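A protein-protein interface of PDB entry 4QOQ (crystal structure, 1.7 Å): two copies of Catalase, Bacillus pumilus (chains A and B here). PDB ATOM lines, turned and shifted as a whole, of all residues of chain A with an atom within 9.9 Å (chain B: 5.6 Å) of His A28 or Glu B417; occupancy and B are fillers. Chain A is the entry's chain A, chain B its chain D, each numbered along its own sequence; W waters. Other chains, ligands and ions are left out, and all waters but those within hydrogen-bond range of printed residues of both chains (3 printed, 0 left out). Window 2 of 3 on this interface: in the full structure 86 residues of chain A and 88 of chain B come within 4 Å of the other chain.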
ATOM      1  N   ASN A  22     -18.039 -28.471  21.629  1.00  0.00           N
ATOM      2  CA  ASN A  22     -19.110 -28.107  20.689  1.00  0.00           C
ATOM      3  C   ASN A  22     -18.896 -28.747  19.316  1.00  0.00           C
ATOM      4  O   ASN A  22     -17.804 -28.645  18.749  1.00  0.00           O
ATOM      5  CB  ASN A  22     -19.156 -26.561  20.512  1.00  0.00           C
ATOM      6  CG  ASN A  22     -19.326 -25.838  21.820  1.00  0.00           C
ATOM      7  OD1 ASN A  22     -20.385 -25.965  22.460  1.00  0.00           O
ATOM      8  ND2 ASN A  22     -18.306 -25.109  22.237  1.00  0.00           N
ATOM      9  N   SER A  23     -19.971 -29.308  18.808  1.00  0.00           N
ATOM     10  CA  SER A  23     -20.091 -29.751  17.437  1.00  0.00           C
ATOM     11  C   SER A  23     -20.059 -28.561  16.525  1.00  0.00           C
ATOM     12  O   SER A  23     -20.366 -27.392  16.914  1.00  0.00           O
ATOM     13  CB  SER A  23     -21.419 -30.500  17.233  1.00  0.00           C
ATOM     14  OG  SER A  23     -21.452 -31.654  18.031  1.00  0.00           O
ATOM     15  N   ARG A  24     -19.738 -28.827  15.268  1.00  0.00           N
ATOM     16  CA  ARG A  24     -19.729 -27.765  14.288  1.00  0.00           C
ATOM     17  C   ARG A  24     -21.093 -27.662  13.628  1.00  0.00           C
ATOM     18  O   ARG A  24     -21.602 -28.638  13.046  1.00  0.00           O
ATOM     19  CB  ARG A  24     -18.682 -28.152  13.240  1.00  0.00           C
ATOM     20  CG  ARG A  24     -18.221 -26.984  12.436  1.00  0.00           C
ATOM     21  CD  ARG A  24     -17.072 -27.477  11.551  1.00  0.00           C
ATOM     22  NE  ARG A  24     -16.397 -26.346  10.983  1.00  0.00           N
ATOM     23  CZ  ARG A  24     -15.708 -26.366   9.842  1.00  0.00           C
ATOM     24  NH1 ARG A  24     -15.598 -27.471   9.139  1.00  0.00           N
ATOM     25  NH2 ARG A  24     -15.124 -25.248   9.430  1.00  0.00           N
ATOM     26  N   THR A  25     -21.662 -26.480  13.647  1.00  0.00           N
ATOM     27  CA  THR A  25     -23.058 -26.281  13.342  1.00  0.00           C
ATOM     28  C   THR A  25     -23.262 -25.024  12.544  1.00  0.00           C
ATOM     29  O   THR A  25     -22.400 -24.163  12.462  1.00  0.00           O
ATOM     30  CB  THR A  25     -23.889 -26.180  14.649  1.00  0.00           C
ATOM     31  OG1 THR A  25     -23.444 -25.057  15.479  1.00  0.00           O
ATOM     32  CG2 THR A  25     -23.786 -27.454  15.444  1.00  0.00           C
ATOM     33  N   ALA A  26     -24.447 -24.917  11.968  1.00  0.00           N
ATOM     34  CA  ALA A  26     -24.879 -23.703  11.286  1.00  0.00           C
ATOM     35  C   ALA A  26     -25.340 -22.632  12.247  1.00  0.00           C
ATOM     36  O   ALA A  26     -26.531 -22.555  12.600  1.00  0.00           O
ATOM     37  CB  ALA A  26     -25.978 -24.027  10.307  1.00  0.00           C
ATOM     38  N   GLY A  27     -24.433 -21.745  12.604  1.00  0.00           N
ATOM     39  CA  GLY A  27     -24.674 -20.813  13.734  1.00  0.00           C
ATOM     40  C   GLY A  27     -24.784 -21.513  15.068  1.00  0.00           C
ATOM     41  O   GLY A  27     -24.634 -22.750  15.158  1.00  0.00           O
ATOM     42  N   HIS A  28     -24.997 -20.741  16.128  1.00  0.00           N
ATOM     43  CA  HIS A  28     -24.819 -21.273  17.484  1.00  0.00           C
ATOM     44  C   HIS A  28     -25.875 -22.325  17.858  1.00  0.00           C
ATOM     45  O   HIS A  28     -25.660 -23.112  18.797  1.00  0.00           O
ATOM     46  CB  HIS A  28     -24.853 -20.142  18.524  1.00  0.00           C
ATOM     47  CG  HIS A  28     -26.201 -19.489  18.653  1.00  0.00           C
ATOM     48  ND1 HIS A  28     -27.203 -19.974  19.486  1.00  0.00           N
ATOM     49  CD2 HIS A  28     -26.717 -18.391  18.053  1.00  0.00           C
ATOM     50  CE1 HIS A  28     -28.279 -19.219  19.372  1.00  0.00           C
ATOM     51  NE2 HIS A  28     -28.013 -18.249  18.507  1.00  0.00           N
ATOM     52  N   ARG A  29     -27.010 -22.369  17.138  1.00  0.00           N
ATOM     53  CA  ARG A  29     -28.076 -23.324  17.447  1.00  0.00           C
ATOM     54  C   ARG A  29     -28.597 -24.102  16.239  1.00  0.00           C
ATOM     55  O   ARG A  29     -29.623 -24.780  16.332  1.00  0.00           O
ATOM     56  CB  ARG A  29     -29.255 -22.624  18.130  1.00  0.00           C
ATOM     57  CG  ARG A  29     -29.997 -21.638  17.270  1.00  0.00           C
ATOM     58  CD  ARG A  29     -31.246 -21.153  17.973  1.00  0.00           C
ATOM     59  NE  ARG A  29     -32.071 -22.258  18.494  1.00  0.00           N
ATOM     60  CZ  ARG A  29     -32.944 -23.006  17.819  1.00  0.00           C
ATOM     61  NH1 ARG A  29     -33.179 -22.851  16.505  1.00  0.00           N
ATOM     62  NH2 ARG A  29     -33.619 -23.982  18.494  1.00  0.00           N
ATOM     63  N   GLY A  30     -27.847 -24.108  15.137  1.00  0.00           N
ATOM     64  CA  GLY A  30     -28.326 -24.792  13.959  1.00  0.00           C
ATOM     65  C   GLY A  30     -27.868 -26.255  13.936  1.00  0.00           C
ATOM     66  O   GLY A  30     -27.242 -26.779  14.859  1.00  0.00           O
ATOM     67  N   PRO A  31     -28.267 -26.974  12.877  1.00  0.00           N
ATOM     68  CA  PRO A  31     -27.970 -28.365  12.745  1.00  0.00           C
ATOM     69  C   PRO A  31     -26.486 -28.581  12.481  1.00  0.00           C
ATOM     70  O   PRO A  31     -25.762 -27.614  12.143  1.00  0.00           O
ATOM     71  CB  PRO A  31     -28.820 -28.782  11.575  1.00  0.00           C
ATOM     72  CG  PRO A  31     -29.147 -27.547  10.826  1.00  0.00           C
ATOM     73  CD  PRO A  31     -29.078 -26.452  11.779  1.00  0.00           C
ATOM     74  N   SER A  32     -26.034 -29.844  12.631  1.00  0.00           N
ATOM     75  CA  SER A  32     -24.628 -30.190  12.600  1.00  0.00           C
ATOM     76  C   SER A  32     -24.129 -30.475  11.157  1.00  0.00           C
ATOM     77  O   SER A  32     -24.849 -31.015  10.318  1.00  0.00           O
ATOM     78  CB  SER A  32     -24.381 -31.380  13.535  1.00  0.00           C
ATOM     79  OG  SER A  32     -24.713 -31.023  14.877  1.00  0.00           O
ATOM     80  N   PHE A  33     -22.898 -30.078  10.894  1.00  0.00           N
ATOM     81  CA  PHE A  33     -22.227 -30.331   9.653  1.00  0.00           C
ATOM     82  C   PHE A  33     -21.516 -31.704   9.642  1.00  0.00           C
ATOM     83  O   PHE A  33     -20.955 -32.180  10.666  1.00  0.00           O
ATOM     84  CB  PHE A  33     -21.267 -29.238   9.374  1.00  0.00           C
ATOM     85  CG  PHE A  33     -21.931 -27.980   8.902  1.00  0.00           C
ATOM     86  CD1 PHE A  33     -22.609 -27.984   7.690  1.00  0.00           C
ATOM     87  CD2 PHE A  33     -21.971 -26.852   9.704  1.00  0.00           C
ATOM     88  CE1 PHE A  33     -23.219 -26.808   7.230  1.00  0.00           C
ATOM     89  CE2 PHE A  33     -22.620 -25.716   9.267  1.00  0.00           C
ATOM     90  CZ  PHE A  33     -23.272 -25.726   8.071  1.00  0.00           C
ATOM     91  N   TYR B 271     -39.585 -19.256  19.984  1.00  0.00           N
ATOM     92  CA  TYR B 271     -38.228 -19.149  20.455  1.00  0.00           C
ATOM     93  C   TYR B 271     -37.970 -17.879  21.273  1.00  0.00           C
ATOM     94  O   TYR B 271     -37.365 -17.944  22.338  1.00  0.00           O
ATOM     95  CB  TYR B 271     -37.205 -19.313  19.292  1.00  0.00           C
ATOM     96  CG  TYR B 271     -35.763 -19.127  19.694  1.00  0.00           C
ATOM     97  CD1 TYR B 271     -35.163 -17.871  19.710  1.00  0.00           C
ATOM     98  CD2 TYR B 271     -35.000 -20.212  20.097  1.00  0.00           C
ATOM     99  CE1 TYR B 271     -33.851 -17.712  20.113  1.00  0.00           C
ATOM    100  CE2 TYR B 271     -33.663 -20.068  20.487  1.00  0.00           C
ATOM    101  CZ  TYR B 271     -33.077 -18.842  20.471  1.00  0.00           C
ATOM    102  OH  TYR B 271     -31.815 -18.654  20.891  1.00  0.00           O
ATOM    103  N   ASP B 277     -33.782 -22.336  25.307  1.00  0.00           N
ATOM    104  CA  ASP B 277     -33.863 -22.792  23.916  1.00  0.00           C
ATOM    105  C   ASP B 277     -34.759 -24.008  23.887  1.00  0.00           C
ATOM    106  O   ASP B 277     -34.464 -24.970  24.590  1.00  0.00           O
ATOM    107  CB  ASP B 277     -32.466 -23.158  23.407  1.00  0.00           C
ATOM    108  CG  ASP B 277     -32.433 -23.476  21.911  1.00  0.00           C
ATOM    109  OD1 ASP B 277     -33.407 -24.066  21.384  1.00  0.00           O
ATOM    110  OD2 ASP B 277     -31.378 -23.120  21.279  1.00  0.00           O
ATOM    111  N   LYS B 331     -28.529 -30.368  19.230  1.00  0.00           N
ATOM    112  CA  LYS B 331     -27.205 -30.783  18.811  1.00  0.00           C
ATOM    113  C   LYS B 331     -26.886 -32.126  19.405  1.00  0.00           C
ATOM    114  O   LYS B 331     -25.987 -32.849  18.955  1.00  0.00           O
ATOM    115  CB  LYS B 331     -26.115 -29.837  19.275  1.00  0.00           C
ATOM    116  CG  LYS B 331     -26.230 -28.421  18.761  1.00  0.00           C
ATOM    117  CD  LYS B 331     -25.052 -27.572  19.211  1.00  0.00           C
ATOM    118  CE  LYS B 331     -25.302 -26.088  18.935  1.00  0.00           C
ATOM    119  NZ  LYS B 331     -24.135 -25.306  19.399  1.00  0.00           N
ATOM    120  N   GLY B 408     -27.995 -19.039  11.334  1.00  0.00           N
ATOM    121  CA  GLY B 408     -26.590 -18.667  11.380  1.00  0.00           C
ATOM    122  C   GLY B 408     -26.007 -18.504   9.991  1.00  0.00           C
ATOM    123  O   GLY B 408     -26.490 -19.114   9.021  1.00  0.00           O
ATOM    124  N   VAL B 412     -19.764 -22.754  12.779  1.00  0.00           N
ATOM    125  CA  VAL B 412     -19.217 -22.418  14.051  1.00  0.00           C
ATOM    126  C   VAL B 412     -19.174 -23.635  15.018  1.00  0.00           C
ATOM    127  O   VAL B 412     -20.013 -24.570  14.934  1.00  0.00           O
ATOM    128  CB  VAL B 412     -19.931 -21.250  14.698  1.00  0.00           C
ATOM    129  CG1 VAL B 412     -19.950 -20.056  13.771  1.00  0.00           C
ATOM    130  CG2 VAL B 412     -21.308 -21.621  15.240  1.00  0.00           C
ATOM    131  N   GLN B 414     -19.880 -23.453  18.901  1.00  0.00           N
ATOM    132  CA  GLN B 414     -20.258 -22.476  19.869  1.00  0.00           C
ATOM    133  C   GLN B 414     -21.439 -22.945  20.660  1.00  0.00           C
ATOM    134  O   GLN B 414     -22.414 -23.419  20.072  1.00  0.00           O
ATOM    135  CB  GLN B 414     -20.666 -21.199  19.104  1.00  0.00           C
ATOM    136  CG  GLN B 414     -20.966 -19.986  19.932  1.00  0.00           C
ATOM    137  CD  GLN B 414     -21.411 -18.813  19.015  1.00  0.00           C
ATOM    138  OE1 GLN B 414     -21.214 -18.850  17.795  1.00  0.00           O
ATOM    139  NE2 GLN B 414     -22.027 -17.820  19.596  1.00  0.00           N
ATOM    140  N   LYS B 415     -21.408 -22.715  21.976  1.00  0.00           N
ATOM    141  CA  LYS B 415     -22.578 -23.072  22.805  1.00  0.00           C
ATOM    142  C   LYS B 415     -23.828 -22.302  22.363  1.00  0.00           C
ATOM    143  O   LYS B 415     -23.752 -21.140  21.955  1.00  0.00           O
ATOM    144  CB  LYS B 415     -22.269 -22.879  24.307  1.00  0.00           C
ATOM    145  CG  LYS B 415     -23.349 -23.473  25.208  1.00  0.00           C
ATOM    146  CD  LYS B 415     -23.264 -23.024  26.636  1.00  0.00           C
ATOM    147  CE  LYS B 415     -21.901 -23.192  27.234  1.00  0.00           C
ATOM    148  NZ  LYS B 415     -22.022 -22.809  28.701  1.00  0.00           N
ATOM    149  N   ILE B 416     -24.994 -22.913  22.491  1.00  0.00           N
ATOM    150  CA  ILE B 416     -26.239 -22.165  22.314  1.00  0.00           C
ATOM    151  C   ILE B 416     -26.268 -20.939  23.226  1.00  0.00           C
ATOM    152  O   ILE B 416     -25.725 -20.940  24.348  1.00  0.00           O
ATOM    153  CB  ILE B 416     -27.495 -23.038  22.605  1.00  0.00           C
ATOM    154  CG1 ILE B 416     -27.447 -23.625  24.013  1.00  0.00           C
ATOM    155  CG2 ILE B 416     -27.642 -24.173  21.560  1.00  0.00           C
ATOM    156  CD1 ILE B 416     -28.801 -24.149  24.477  1.00  0.00           C
ATOM    157  N   GLU B 417     -27.010 -19.935  22.762  1.00  0.00           N
ATOM    158  CA  GLU B 417     -27.463 -18.854  23.604  1.00  0.00           C
ATOM    159  C   GLU B 417     -28.504 -19.367  24.618  1.00  0.00           C
ATOM    160  O   GLU B 417     -29.181 -20.348  24.395  1.00  0.00           O
ATOM    161  CB  GLU B 417     -27.998 -17.681  22.754  1.00  0.00           C
ATOM    162  CG  GLU B 417     -26.881 -16.892  22.081  1.00  0.00           C
ATOM    163  CD  GLU B 417     -27.303 -16.067  20.852  1.00  0.00           C
ATOM    164  OE1 GLU B 417     -28.264 -15.274  20.924  1.00  0.00           O
ATOM    165  OE2 GLU B 417     -26.623 -16.179  19.801  1.00  0.00           O
ATOM    166  N   LYS B 418     -28.636 -18.623  25.715  1.00  0.00           N
ATOM    167  CA  LYS B 418     -29.559 -18.908  26.804  1.00  0.00           C
ATOM    168  C   LYS B 418     -29.514 -20.378  27.292  1.00  0.00           C
ATOM    169  O   LYS B 418     -30.551 -21.015  27.460  1.00  0.00           O
ATOM    170  CB  LYS B 418     -30.938 -18.377  26.550  1.00  0.00           C
ATOM    171  CG  LYS B 418     -31.632 -18.759  25.270  1.00  0.00           C
ATOM    172  CD  LYS B 418     -33.033 -18.218  25.191  1.00  0.00           C
ATOM    173  CE  LYS B 418     -33.608 -18.618  23.876  1.00  0.00           C
ATOM    174  NZ  LYS B 418     -34.936 -18.033  23.699  1.00  0.00           N
ATOM    175  N   PRO B 419     -28.302 -20.853  27.615  1.00  0.00           N
ATOM    176  CA  PRO B 419     -28.173 -22.145  28.208  1.00  0.00           C
ATOM    177  C   PRO B 419     -28.930 -22.280  29.518  1.00  0.00           C
ATOM    178  O   PRO B 419     -29.540 -23.336  29.759  1.00  0.00           O
ATOM    179  CB  PRO B 419     -26.685 -22.288  28.446  1.00  0.00           C
ATOM    180  CG  PRO B 419     -26.195 -20.873  28.574  1.00  0.00           C
ATOM    181  CD  PRO B 419     -27.020 -20.147  27.571  1.00  0.00           C
HETATM  182  O   HOH W   1     -23.908 -32.792  16.904  1.00  0.00           O
HETATM  183  O   HOH W   2     -22.678 -26.806  21.571  1.00  0.00           O
HETATM  184  O   HOH W   3     -21.821 -25.326  17.570  1.00  0.00           O
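OD1 of Asn A22 sits at hydrogen-bond distance from N of Lys B415 (3.4 Å).
O of Val B412 lies within hydrogen-bond range of N of Thr A25, at 2.8 Å.
The side-chain amino group (NZ) of Lys B331 sits at hydrogen-bond distance from the backbone carbonyl oxygen (O) of His A28, 2.7 Å away.
NE2 of His A28 lies within hydrogen-bond range of OE2 of Glu B417, 2.8 Å away.
The guanidinium group (NH2) of Arg A29 lies within salt-bridge range of the side-chain carboxylate (OD1) of Asp B277 (2.9 Å).
The backbone carbonyl oxygen (O) of Ser A23 lies close to the backbone carbonyl oxygen (O) of Val B412 (3.5 Å).
The backbone carbonyl oxygen (O) of Arg A24 sits at hydrogen-bond distance from the backbone NH (N) of Phe A33 (2.9 Å).
OG1 of Thr A25 sits at hydrogen-bond distance from O of Gly A27.
The backbone carbonyl oxygen (O) of Tyr B271 lies within hydrogen-bond range of the side-chain amino group (NZ) of Lys B418 (2.8 Å).
NZ of Lys B331 sits at hydrogen-bond distance from O of Gln B414, 2.6 Å away.
Among the printed residues, merely in contact across the chains: Arg A24 with Val B412, Arg A29 with Tyr B271, Gly A27 with Val B412, His A28 with Gln B414, His A28 with Ile B416, Asn A22 with Gln B414, Gly A27 with Gly B408, His A28 with Lys B415, His A28 with Tyr B271, His A28 with Val B412 and Thr A25 with Lys B331.
Printed residues of chain B within 4 Å of Thr A25: Lys B331 (3.98 Å) and Val B412 (2.8 Å).
Printed residues of chain B within 4 Å of His A28: Tyr B271, Lys B331, Val B412, Gln B414, Lys B415, Ile B416 and Glu B417.
Pro A31 touches none of the printed residues of chain B.
Of the printed residues of chain A, Gly B408 touches Gly A27 (3.7 Å).
Of the printed residues of chain A, Lys B415 touches Asn A22 and His A28.
Of chain A, only His A28 (3.6 Å) comes within 4 Å of Ile B416.
Printed residues of chain A within 4 Å of Glu B417: His A28 (2.8 Å).
Lys B418 touches none of the printed residues of chain A.
The nearest printed residue of chain B that does not touch His A28 is Asp B277 (5.3 Å).
The nearest printed residue of chain A that does not touch Glu B417 is Arg A29 (5.8 Å).
The nearest printed residue of chain B that does not touch Arg A29 is Ile B416 (4.1 Å).
Of the 11 printed residues of chain B, 9 touch a printed residue of chain A.
Hydrophobic or aromatic side chains of chain B within 4 Å of the printed part of chain A: Tyr B271, Val B412 and Ile B416.
Of the 12 printed residues of chain A, 7 touch a printed residue of chain B.
Hydrophobic or aromatic side chains of chain A that line the printed part of chain B: His A28.
Along chain A the printed residues that touch a printed residue of chain B span positions 22 to 29.
Among the printed residues, Asp or Glu carboxylates within 4 Å of a Lys or Arg side-chain nitrogen of the other chain: Arg A29 with Asp B277 (2.9 Å).
No position is printed for both chains.
Of the 17 pairs that touch across the chains among the printed residues, none has its exchanged pair printed and touching as well.
Water W2 bridges the side-chain amide oxygen of Asn A22 (2.6 Å) and the side-chain amino group of Lys B331 (3.0 Å).
Water W3 lies within hydrogen-bond range of the backbone carbonyl oxygen (O) of Ser A23 (2.6 Å), the side-chain hydroxyl (OG1) of Thr A25 (2.7 Å), the side-chain amino group (NZ) of Lys B331 (2.9 Å), the backbone NH (N) of Gln B414 (3.0 Å) and the backbone carbonyl oxygen (O) of Val B412 (3.3 Å).
Water W1 lies within hydrogen-bond range of the side-chain hydroxyl of Ser A32 (2.8 Å), the backbone carbonyl oxygen of Lys B331 (2.9 Å) and the side-chain hydroxyl of Ser A23 (2.9 Å).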
